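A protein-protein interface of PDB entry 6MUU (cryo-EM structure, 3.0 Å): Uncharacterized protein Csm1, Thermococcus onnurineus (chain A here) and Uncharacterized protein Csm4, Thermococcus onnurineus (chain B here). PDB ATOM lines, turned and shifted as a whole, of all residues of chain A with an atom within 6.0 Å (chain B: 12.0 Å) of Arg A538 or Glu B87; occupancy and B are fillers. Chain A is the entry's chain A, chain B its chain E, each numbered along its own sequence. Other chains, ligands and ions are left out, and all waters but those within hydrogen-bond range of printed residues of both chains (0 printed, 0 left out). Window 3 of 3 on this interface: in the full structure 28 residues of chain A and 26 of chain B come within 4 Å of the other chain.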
ATOM      1  N   VAL A 536      28.128  -9.362  25.341  1.00  0.00           N
ATOM      2  CA  VAL A 536      28.064 -10.756  24.941  1.00  0.00           C
ATOM      3  C   VAL A 536      26.927 -10.900  23.949  1.00  0.00           C
ATOM      4  O   VAL A 536      25.818 -10.408  24.183  1.00  0.00           O
ATOM      5  CB  VAL A 536      27.865 -11.662  26.162  1.00  0.00           C
ATOM      6  CG1 VAL A 536      27.841 -13.108  25.758  1.00  0.00           C
ATOM      7  CG2 VAL A 536      28.962 -11.418  27.128  1.00  0.00           C
ATOM      8  N   ASP A 537      27.204 -11.562  22.841  1.00  0.00           N
ATOM      9  CA  ASP A 537      26.286 -11.621  21.721  1.00  0.00           C
ATOM     10  C   ASP A 537      25.418 -12.869  21.778  1.00  0.00           C
ATOM     11  O   ASP A 537      25.871 -13.930  22.217  1.00  0.00           O
ATOM     12  CB  ASP A 537      27.065 -11.578  20.417  1.00  0.00           C
ATOM     13  CG  ASP A 537      28.154 -12.606  20.359  1.00  0.00           C
ATOM     14  OD1 ASP A 537      28.467 -13.205  21.398  1.00  0.00           O
ATOM     15  OD2 ASP A 537      28.691 -12.844  19.265  1.00  0.00           O
ATOM     16  N   ARG A 538      24.163 -12.711  21.335  1.00  0.00           N
ATOM     17  CA  ARG A 538      23.141 -13.763  21.324  1.00  0.00           C
ATOM     18  C   ARG A 538      22.931 -14.341  22.717  1.00  0.00           C
ATOM     19  O   ARG A 538      22.758 -15.546  22.894  1.00  0.00           O
ATOM     20  CB  ARG A 538      23.482 -14.853  20.309  1.00  0.00           C
ATOM     21  CG  ARG A 538      23.506 -14.343  18.884  1.00  0.00           C
ATOM     22  CD  ARG A 538      24.105 -15.355  17.933  1.00  0.00           C
ATOM     23  NE  ARG A 538      23.303 -16.566  17.806  1.00  0.00           N
ATOM     24  CZ  ARG A 538      22.303 -16.703  16.944  1.00  0.00           C
ATOM     25  NH1 ARG A 538      21.974 -15.706  16.144  1.00  0.00           N
ATOM     26  NH2 ARG A 538      21.626 -17.845  16.892  1.00  0.00           N
ATOM     27  N   LEU A 539      22.954 -13.465  23.716  1.00  0.00           N
ATOM     28  CA  LEU A 539      22.849 -13.894  25.101  1.00  0.00           C
ATOM     29  C   LEU A 539      21.402 -14.111  25.507  1.00  0.00           C
ATOM     30  O   LEU A 539      21.125 -14.942  26.376  1.00  0.00           O
ATOM     31  CB  LEU A 539      23.516 -12.853  25.995  1.00  0.00           C
ATOM     32  CG  LEU A 539      23.645 -13.064  27.496  1.00  0.00           C
ATOM     33  CD1 LEU A 539      24.507 -14.260  27.790  1.00  0.00           C
ATOM     34  CD2 LEU A 539      24.241 -11.821  28.115  1.00  0.00           C
ATOM     35  N   GLY A 540      20.474 -13.377  24.893  1.00  0.00           N
ATOM     36  CA  GLY A 540      19.066 -13.611  25.149  1.00  0.00           C
ATOM     37  C   GLY A 540      18.573 -14.932  24.600  1.00  0.00           C
ATOM     38  O   GLY A 540      17.634 -15.516  25.144  1.00  0.00           O
ATOM     39  N   GLU A 541      19.183 -15.415  23.513  1.00  0.00           N
ATOM     40  CA  GLU A 541      18.901 -16.770  23.052  1.00  0.00           C
ATOM     41  C   GLU A 541      19.381 -17.804  24.052  1.00  0.00           C
ATOM     42  O   GLU A 541      18.698 -18.806  24.289  1.00  0.00           O
ATOM     43  CB  GLU A 541      19.571 -17.053  21.712  1.00  0.00           C
ATOM     44  CG  GLU A 541      18.968 -16.414  20.494  1.00  0.00           C
ATOM     45  CD  GLU A 541      19.646 -16.918  19.239  1.00  0.00           C
ATOM     46  OE1 GLU A 541      20.627 -17.679  19.373  1.00  0.00           O
ATOM     47  OE2 GLU A 541      19.207 -16.580  18.122  1.00  0.00           O
ATOM     48  N   PHE A 542      20.569 -17.587  24.625  1.00  0.00           N
ATOM     49  CA  PHE A 542      21.172 -18.571  25.515  1.00  0.00           C
ATOM     50  C   PHE A 542      20.387 -18.732  26.807  1.00  0.00           C
ATOM     51  O   PHE A 542      20.272 -19.847  27.321  1.00  0.00           O
ATOM     52  CB  PHE A 542      22.620 -18.190  25.813  1.00  0.00           C
ATOM     53  CG  PHE A 542      23.274 -19.075  26.821  1.00  0.00           C
ATOM     54  CD1 PHE A 542      23.574 -20.386  26.514  1.00  0.00           C
ATOM     55  CD2 PHE A 542      23.600 -18.590  28.076  1.00  0.00           C
ATOM     56  CE1 PHE A 542      24.172 -21.203  27.444  1.00  0.00           C
ATOM     57  CE2 PHE A 542      24.198 -19.402  29.008  1.00  0.00           C
ATOM     58  CZ  PHE A 542      24.485 -20.707  28.691  1.00  0.00           C
ATOM     59  N   PHE A 543      19.808 -17.653  27.324  1.00  0.00           N
ATOM     60  CA  PHE A 543      18.980 -17.757  28.514  1.00  0.00           C
ATOM     61  C   PHE A 543      17.608 -18.351  28.229  1.00  0.00           C
ATOM     62  O   PHE A 543      16.891 -18.691  29.175  1.00  0.00           O
ATOM     63  CB  PHE A 543      18.824 -16.382  29.160  1.00  0.00           C
ATOM     64  CG  PHE A 543      20.062 -15.890  29.843  1.00  0.00           C
ATOM     65  CD1 PHE A 543      21.044 -16.773  30.257  1.00  0.00           C
ATOM     66  CD2 PHE A 543      20.254 -14.538  30.050  1.00  0.00           C
ATOM     67  CE1 PHE A 543      22.184 -16.317  30.881  1.00  0.00           C
ATOM     68  CE2 PHE A 543      21.393 -14.079  30.672  1.00  0.00           C
ATOM     69  CZ  PHE A 543      22.357 -14.969  31.084  1.00  0.00           C
ATOM     70  N   LEU A 632      29.881 -18.958  23.335  1.00  0.00           N
ATOM     71  CA  LEU A 632      29.512 -17.554  23.377  1.00  0.00           C
ATOM     72  C   LEU A 632      30.744 -16.706  23.113  1.00  0.00           C
ATOM     73  O   LEU A 632      31.856 -17.063  23.506  1.00  0.00           O
ATOM     74  CB  LEU A 632      28.904 -17.186  24.726  1.00  0.00           C
ATOM     75  CG  LEU A 632      27.546 -17.790  25.059  1.00  0.00           C
ATOM     76  CD1 LEU A 632      27.226 -17.534  26.502  1.00  0.00           C
ATOM     77  CD2 LEU A 632      26.493 -17.154  24.188  1.00  0.00           C
ATOM     78  N   ARG A 666      29.141 -10.207  14.156  1.00  0.00           N
ATOM     79  CA  ARG A 666      28.782 -10.229  15.574  1.00  0.00           C
ATOM     80  C   ARG A 666      29.841 -10.904  16.457  1.00  0.00           C
ATOM     81  O   ARG A 666      29.804 -10.777  17.682  1.00  0.00           O
ATOM     82  CB  ARG A 666      27.391 -10.868  15.723  1.00  0.00           C
ATOM     83  CG  ARG A 666      26.676 -10.623  17.017  1.00  0.00           C
ATOM     84  CD  ARG A 666      25.292 -11.218  17.008  1.00  0.00           C
ATOM     85  NE  ARG A 666      24.385 -10.444  16.171  1.00  0.00           N
ATOM     86  CZ  ARG A 666      23.632  -9.444  16.618  1.00  0.00           C
ATOM     87  NH1 ARG A 666      23.650  -9.122  17.903  1.00  0.00           N
ATOM     88  NH2 ARG A 666      22.838  -8.785  15.786  1.00  0.00           N
ATOM     89  N   LEU B  81       7.118 -11.148  11.745  1.00  0.00           N
ATOM     90  CA  LEU B  81       8.125 -12.074  11.235  1.00  0.00           C
ATOM     91  C   LEU B  81       7.794 -13.525  11.551  1.00  0.00           C
ATOM     92  O   LEU B  81       8.688 -14.312  11.871  1.00  0.00           O
ATOM     93  CB  LEU B  81       9.500 -11.707  11.780  1.00  0.00           C
ATOM     94  CG  LEU B  81      10.012 -10.336  11.342  1.00  0.00           C
ATOM     95  CD1 LEU B  81      11.368 -10.063  11.952  1.00  0.00           C
ATOM     96  CD2 LEU B  81      10.063 -10.230   9.832  1.00  0.00           C
ATOM     97  N   THR B  82       6.511 -13.898  11.489  1.00  0.00           N
ATOM     98  CA  THR B  82       6.130 -15.298  11.673  1.00  0.00           C
ATOM     99  C   THR B  82       6.617 -16.162  10.519  1.00  0.00           C
ATOM    100  O   THR B  82       7.004 -17.318  10.720  1.00  0.00           O
ATOM    101  CB  THR B  82       4.613 -15.422  11.812  1.00  0.00           C
ATOM    102  OG1 THR B  82       3.983 -14.906  10.633  1.00  0.00           O
ATOM    103  CG2 THR B  82       4.122 -14.653  13.023  1.00  0.00           C
ATOM    104  N   GLY B  83       6.597 -15.624   9.304  1.00  0.00           N
ATOM    105  CA  GLY B  83       7.089 -16.356   8.157  1.00  0.00           C
ATOM    106  C   GLY B  83       8.562 -16.120   7.916  1.00  0.00           C
ATOM    107  O   GLY B  83       8.940 -15.503   6.917  1.00  0.00           O
ATOM    108  N   LEU B  84       9.401 -16.607   8.829  1.00  0.00           N
ATOM    109  CA  LEU B  84      10.842 -16.437   8.710  1.00  0.00           C
ATOM    110  C   LEU B  84      11.509 -17.557   9.495  1.00  0.00           C
ATOM    111  O   LEU B  84      10.920 -18.131  10.414  1.00  0.00           O
ATOM    112  CB  LEU B  84      11.273 -15.047   9.204  1.00  0.00           C
ATOM    113  CG  LEU B  84      12.627 -14.446   8.814  1.00  0.00           C
ATOM    114  CD1 LEU B  84      12.481 -12.946   8.681  1.00  0.00           C
ATOM    115  CD2 LEU B  84      13.710 -14.744   9.822  1.00  0.00           C
ATOM    116  N   ASP B  85      12.740 -17.873   9.100  1.00  0.00           N
ATOM    117  CA  ASP B  85      13.474 -18.992   9.680  1.00  0.00           C
ATOM    118  C   ASP B  85      13.889 -18.682  11.113  1.00  0.00           C
ATOM    119  O   ASP B  85      14.545 -17.670  11.371  1.00  0.00           O
ATOM    120  CB  ASP B  85      14.702 -19.293   8.827  1.00  0.00           C
ATOM    121  CG  ASP B  85      14.340 -19.741   7.424  1.00  0.00           C
ATOM    122  OD1 ASP B  85      13.269 -20.361   7.252  1.00  0.00           O
ATOM    123  OD2 ASP B  85      15.120 -19.458   6.492  1.00  0.00           O
ATOM    124  N   GLU B  86      13.540 -19.581  12.040  1.00  0.00           N
ATOM    125  CA  GLU B  86      13.655 -19.305  13.471  1.00  0.00           C
ATOM    126  C   GLU B  86      15.089 -19.283  13.982  1.00  0.00           C
ATOM    127  O   GLU B  86      15.308 -18.880  15.127  1.00  0.00           O
ATOM    128  CB  GLU B  86      12.847 -20.322  14.278  1.00  0.00           C
ATOM    129  CG  GLU B  86      11.339 -20.157  14.159  1.00  0.00           C
ATOM    130  CD  GLU B  86      10.755 -20.879  12.963  1.00  0.00           C
ATOM    131  OE1 GLU B  86      11.508 -21.600  12.272  1.00  0.00           O
ATOM    132  OE2 GLU B  86       9.543 -20.721  12.710  1.00  0.00           O
ATOM    133  N   GLU B  87      16.062 -19.700  13.179  1.00  0.00           N
ATOM    134  CA  GLU B  87      17.451 -19.568  13.592  1.00  0.00           C
ATOM    135  C   GLU B  87      17.952 -18.145  13.411  1.00  0.00           C
ATOM    136  O   GLU B  87      18.932 -17.751  14.052  1.00  0.00           O
ATOM    137  CB  GLU B  87      18.329 -20.552  12.814  1.00  0.00           C
ATOM    138  CG  GLU B  87      18.098 -22.017  13.175  1.00  0.00           C
ATOM    139  CD  GLU B  87      16.949 -22.648  12.411  1.00  0.00           C
ATOM    140  OE1 GLU B  87      16.386 -21.981  11.516  1.00  0.00           O
ATOM    141  OE2 GLU B  87      16.602 -23.808  12.712  1.00  0.00           O
ATOM    142  N   GLU B  88      17.297 -17.366  12.551  1.00  0.00           N
ATOM    143  CA  GLU B  88      17.676 -15.981  12.302  1.00  0.00           C
ATOM    144  C   GLU B  88      16.540 -14.998  12.555  1.00  0.00           C
ATOM    145  O   GLU B  88      16.634 -13.843  12.128  1.00  0.00           O
ATOM    146  CB  GLU B  88      18.195 -15.824  10.869  1.00  0.00           C
ATOM    147  CG  GLU B  88      17.171 -16.129   9.794  1.00  0.00           C
ATOM    148  CD  GLU B  88      17.738 -16.008   8.389  1.00  0.00           C
ATOM    149  OE1 GLU B  88      18.942 -15.705   8.254  1.00  0.00           O
ATOM    150  OE2 GLU B  88      16.981 -16.218   7.419  1.00  0.00           O
ATOM    151  N   ARG B  89      15.466 -15.419  13.230  1.00  0.00           N
ATOM    152  CA  ARG B  89      14.440 -14.464  13.634  1.00  0.00           C
ATOM    153  C   ARG B  89      14.948 -13.520  14.710  1.00  0.00           C
ATOM    154  O   ARG B  89      14.497 -12.375  14.786  1.00  0.00           O
ATOM    155  CB  ARG B  89      13.190 -15.180  14.143  1.00  0.00           C
ATOM    156  CG  ARG B  89      12.354 -15.841  13.076  1.00  0.00           C
ATOM    157  CD  ARG B  89      11.120 -16.482  13.677  1.00  0.00           C
ATOM    158  NE  ARG B  89      10.220 -15.484  14.244  1.00  0.00           N
ATOM    159  CZ  ARG B  89       9.146 -15.770  14.971  1.00  0.00           C
ATOM    160  NH1 ARG B  89       8.828 -17.031  15.224  1.00  0.00           N
ATOM    161  NH2 ARG B  89       8.388 -14.793  15.448  1.00  0.00           N
ATOM    162  N   TYR B  90      15.889 -13.979  15.536  1.00  0.00           N
ATOM    163  CA  TYR B  90      16.358 -13.201  16.675  1.00  0.00           C
ATOM    164  C   TYR B  90      17.232 -12.033  16.238  1.00  0.00           C
ATOM    165  O   TYR B  90      17.044 -10.905  16.704  1.00  0.00           O
ATOM    166  CB  TYR B  90      17.117 -14.115  17.632  1.00  0.00           C
ATOM    167  CG  TYR B  90      17.606 -13.462  18.903  1.00  0.00           C
ATOM    168  CD1 TYR B  90      16.728 -13.184  19.944  1.00  0.00           C
ATOM    169  CD2 TYR B  90      18.948 -13.143  19.070  1.00  0.00           C
ATOM    170  CE1 TYR B  90      17.172 -12.597  21.115  1.00  0.00           C
ATOM    171  CE2 TYR B  90      19.403 -12.562  20.237  1.00  0.00           C
ATOM    172  CZ  TYR B  90      18.510 -12.288  21.256  1.00  0.00           C
ATOM    173  OH  TYR B  90      18.957 -11.703  22.419  1.00  0.00           O
ATOM    174  N   THR B  91      18.198 -12.283  15.351  1.00  0.00           N
ATOM    175  CA  THR B  91      19.063 -11.200  14.895  1.00  0.00           C
ATOM    176  C   THR B  91      18.340 -10.268  13.941  1.00  0.00           C
ATOM    177  O   THR B  91      18.680  -9.083  13.860  1.00  0.00           O
ATOM    178  CB  THR B  91      20.309 -11.752  14.215  1.00  0.00           C
ATOM    179  OG1 THR B  91      19.926 -12.545  13.085  1.00  0.00           O
ATOM    180  CG2 THR B  91      21.105 -12.591  15.185  1.00  0.00           C
ATOM    181  N   THR B  92      17.356 -10.785  13.204  1.00  0.00           N
ATOM    182  CA  THR B  92      16.527  -9.917  12.380  1.00  0.00           C
ATOM    183  C   THR B  92      15.674  -9.007  13.247  1.00  0.00           C
ATOM    184  O   THR B  92      15.449  -7.851  12.887  1.00  0.00           O
ATOM    185  CB  THR B  92      15.645 -10.761  11.457  1.00  0.00           C
ATOM    186  OG1 THR B  92      16.464 -11.692  10.741  1.00  0.00           O
ATOM    187  CG2 THR B  92      14.919  -9.889  10.444  1.00  0.00           C
ATOM    188  N   ALA B  93      15.245  -9.493  14.414  1.00  0.00           N
ATOM    189  CA  ALA B  93      14.333  -8.731  15.259  1.00  0.00           C
ATOM    190  C   ALA B  93      15.003  -7.507  15.860  1.00  0.00           C
ATOM    191  O   ALA B  93      14.495  -6.389  15.732  1.00  0.00           O
ATOM    192  CB  ALA B  93      13.768  -9.617  16.366  1.00  0.00           C
ATOM    193  N   LYS B  94      16.146  -7.695  16.519  1.00  0.00           N
ATOM    194  CA  LYS B  94      16.784  -6.573  17.196  1.00  0.00           C
ATOM    195  C   LYS B  94      17.435  -5.602  16.222  1.00  0.00           C
ATOM    196  O   LYS B  94      17.592  -4.426  16.551  1.00  0.00           O
ATOM    197  CB  LYS B  94      17.811  -7.071  18.208  1.00  0.00           C
ATOM    198  CG  LYS B  94      18.922  -7.901  17.621  1.00  0.00           C
ATOM    199  CD  LYS B  94      19.979  -8.149  18.667  1.00  0.00           C
ATOM    200  CE  LYS B  94      19.457  -9.042  19.766  1.00  0.00           C
ATOM    201  NZ  LYS B  94      20.540  -9.393  20.727  1.00  0.00           N
ATOM    202  N   ARG B  95      17.816  -6.061  15.029  1.00  0.00           N
ATOM    203  CA  ARG B  95      18.340  -5.133  14.033  1.00  0.00           C
ATOM    204  C   ARG B  95      17.234  -4.264  13.463  1.00  0.00           C
ATOM    205  O   ARG B  95      17.456  -3.088  13.158  1.00  0.00           O
ATOM    206  CB  ARG B  95      19.035  -5.902  12.911  1.00  0.00           C
ATOM    207  CG  ARG B  95      19.760  -5.029  11.905  1.00  0.00           C
ATOM    208  CD  ARG B  95      20.355  -5.860  10.791  1.00  0.00           C
ATOM    209  NE  ARG B  95      19.312  -6.492   9.991  1.00  0.00           N
ATOM    210  CZ  ARG B  95      19.112  -7.804   9.935  1.00  0.00           C
ATOM    211  NH1 ARG B  95      19.887  -8.621  10.635  1.00  0.00           N
ATOM    212  NH2 ARG B  95      18.138  -8.298   9.185  1.00  0.00           N
ATOM    213  N   ARG B  97      14.509  -3.591  15.206  1.00  0.00           N
ATOM    214  CA  ARG B  97      13.946  -2.845  16.324  1.00  0.00           C
ATOM    215  C   ARG B  97      14.718  -1.560  16.594  1.00  0.00           C
ATOM    216  O   ARG B  97      14.115  -0.498  16.763  1.00  0.00           O
ATOM    217  CB  ARG B  97      13.915  -3.714  17.583  1.00  0.00           C
ATOM    218  CG  ARG B  97      13.332  -3.016  18.791  1.00  0.00           C
ATOM    219  CD  ARG B  97      13.244  -3.929  20.000  1.00  0.00           C
ATOM    220  NE  ARG B  97      12.270  -4.999  19.814  1.00  0.00           N
ATOM    221  CZ  ARG B  97      12.575  -6.290  19.767  1.00  0.00           C
ATOM    222  NH1 ARG B  97      11.618  -7.188  19.595  1.00  0.00           N
ATOM    223  NH2 ARG B  97      13.834  -6.683  19.902  1.00  0.00           N
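The side-chain hydroxyl of Tyr B90 lies close to the backbone NH of Gly A540, at 3.4 Å.
NH2 of Arg A538 lies within salt-bridge range of OE1 of Glu A541 (2.7 Å).
The side-chain amino group of Lys B94 lies within hydrogen-bond range of the side-chain hydroxyl of Tyr B90 (3.3 Å).
The guanidinium group of Arg B95 lies close to the backbone carbonyl oxygen of Thr B91, at 3.5 Å.
Arg A538 touches Glu B87.
Thr B91 touches Arg A538.
CB of Tyr B90 touches OE2 of Glu A541 (3.3 Å).
Arg A666 touches Lys B94 (NH1 to CD, 3.9 Å).
No residue of chain B comes within 4 Å of Asp A537.
Of chain B, only Glu B87 (3.9 Å) and Thr B91 (3.4 Å) come within 4 Å of Arg A538.
Phe A542 touches none of the printed residues of chain B.
Thr B82 touches none of the printed residues of chain A.
Glu B87 touches just one residue of chain A: Arg A538.
Of the printed residues of chain A, Tyr B90 touches Gly A540 (3.3 Å) and Glu A541 (3.3 Å).
Printed residues of chain A within 4 Å of Thr B91: Arg A538.
Of the printed residues of chain A, Lys B94 touches Arg A666 (3.9 Å).
The nearest residue of chain A that does not touch Glu B87 is Glu A541 (4.2 Å).
Of the 10 printed residues of chain A, 4 touch a printed residue of chain B.
Along chain B the printed residues that touch a printed residue of chain A span positions 87 to 94.
Among the printed residues, 5 pairs touch across the chains.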
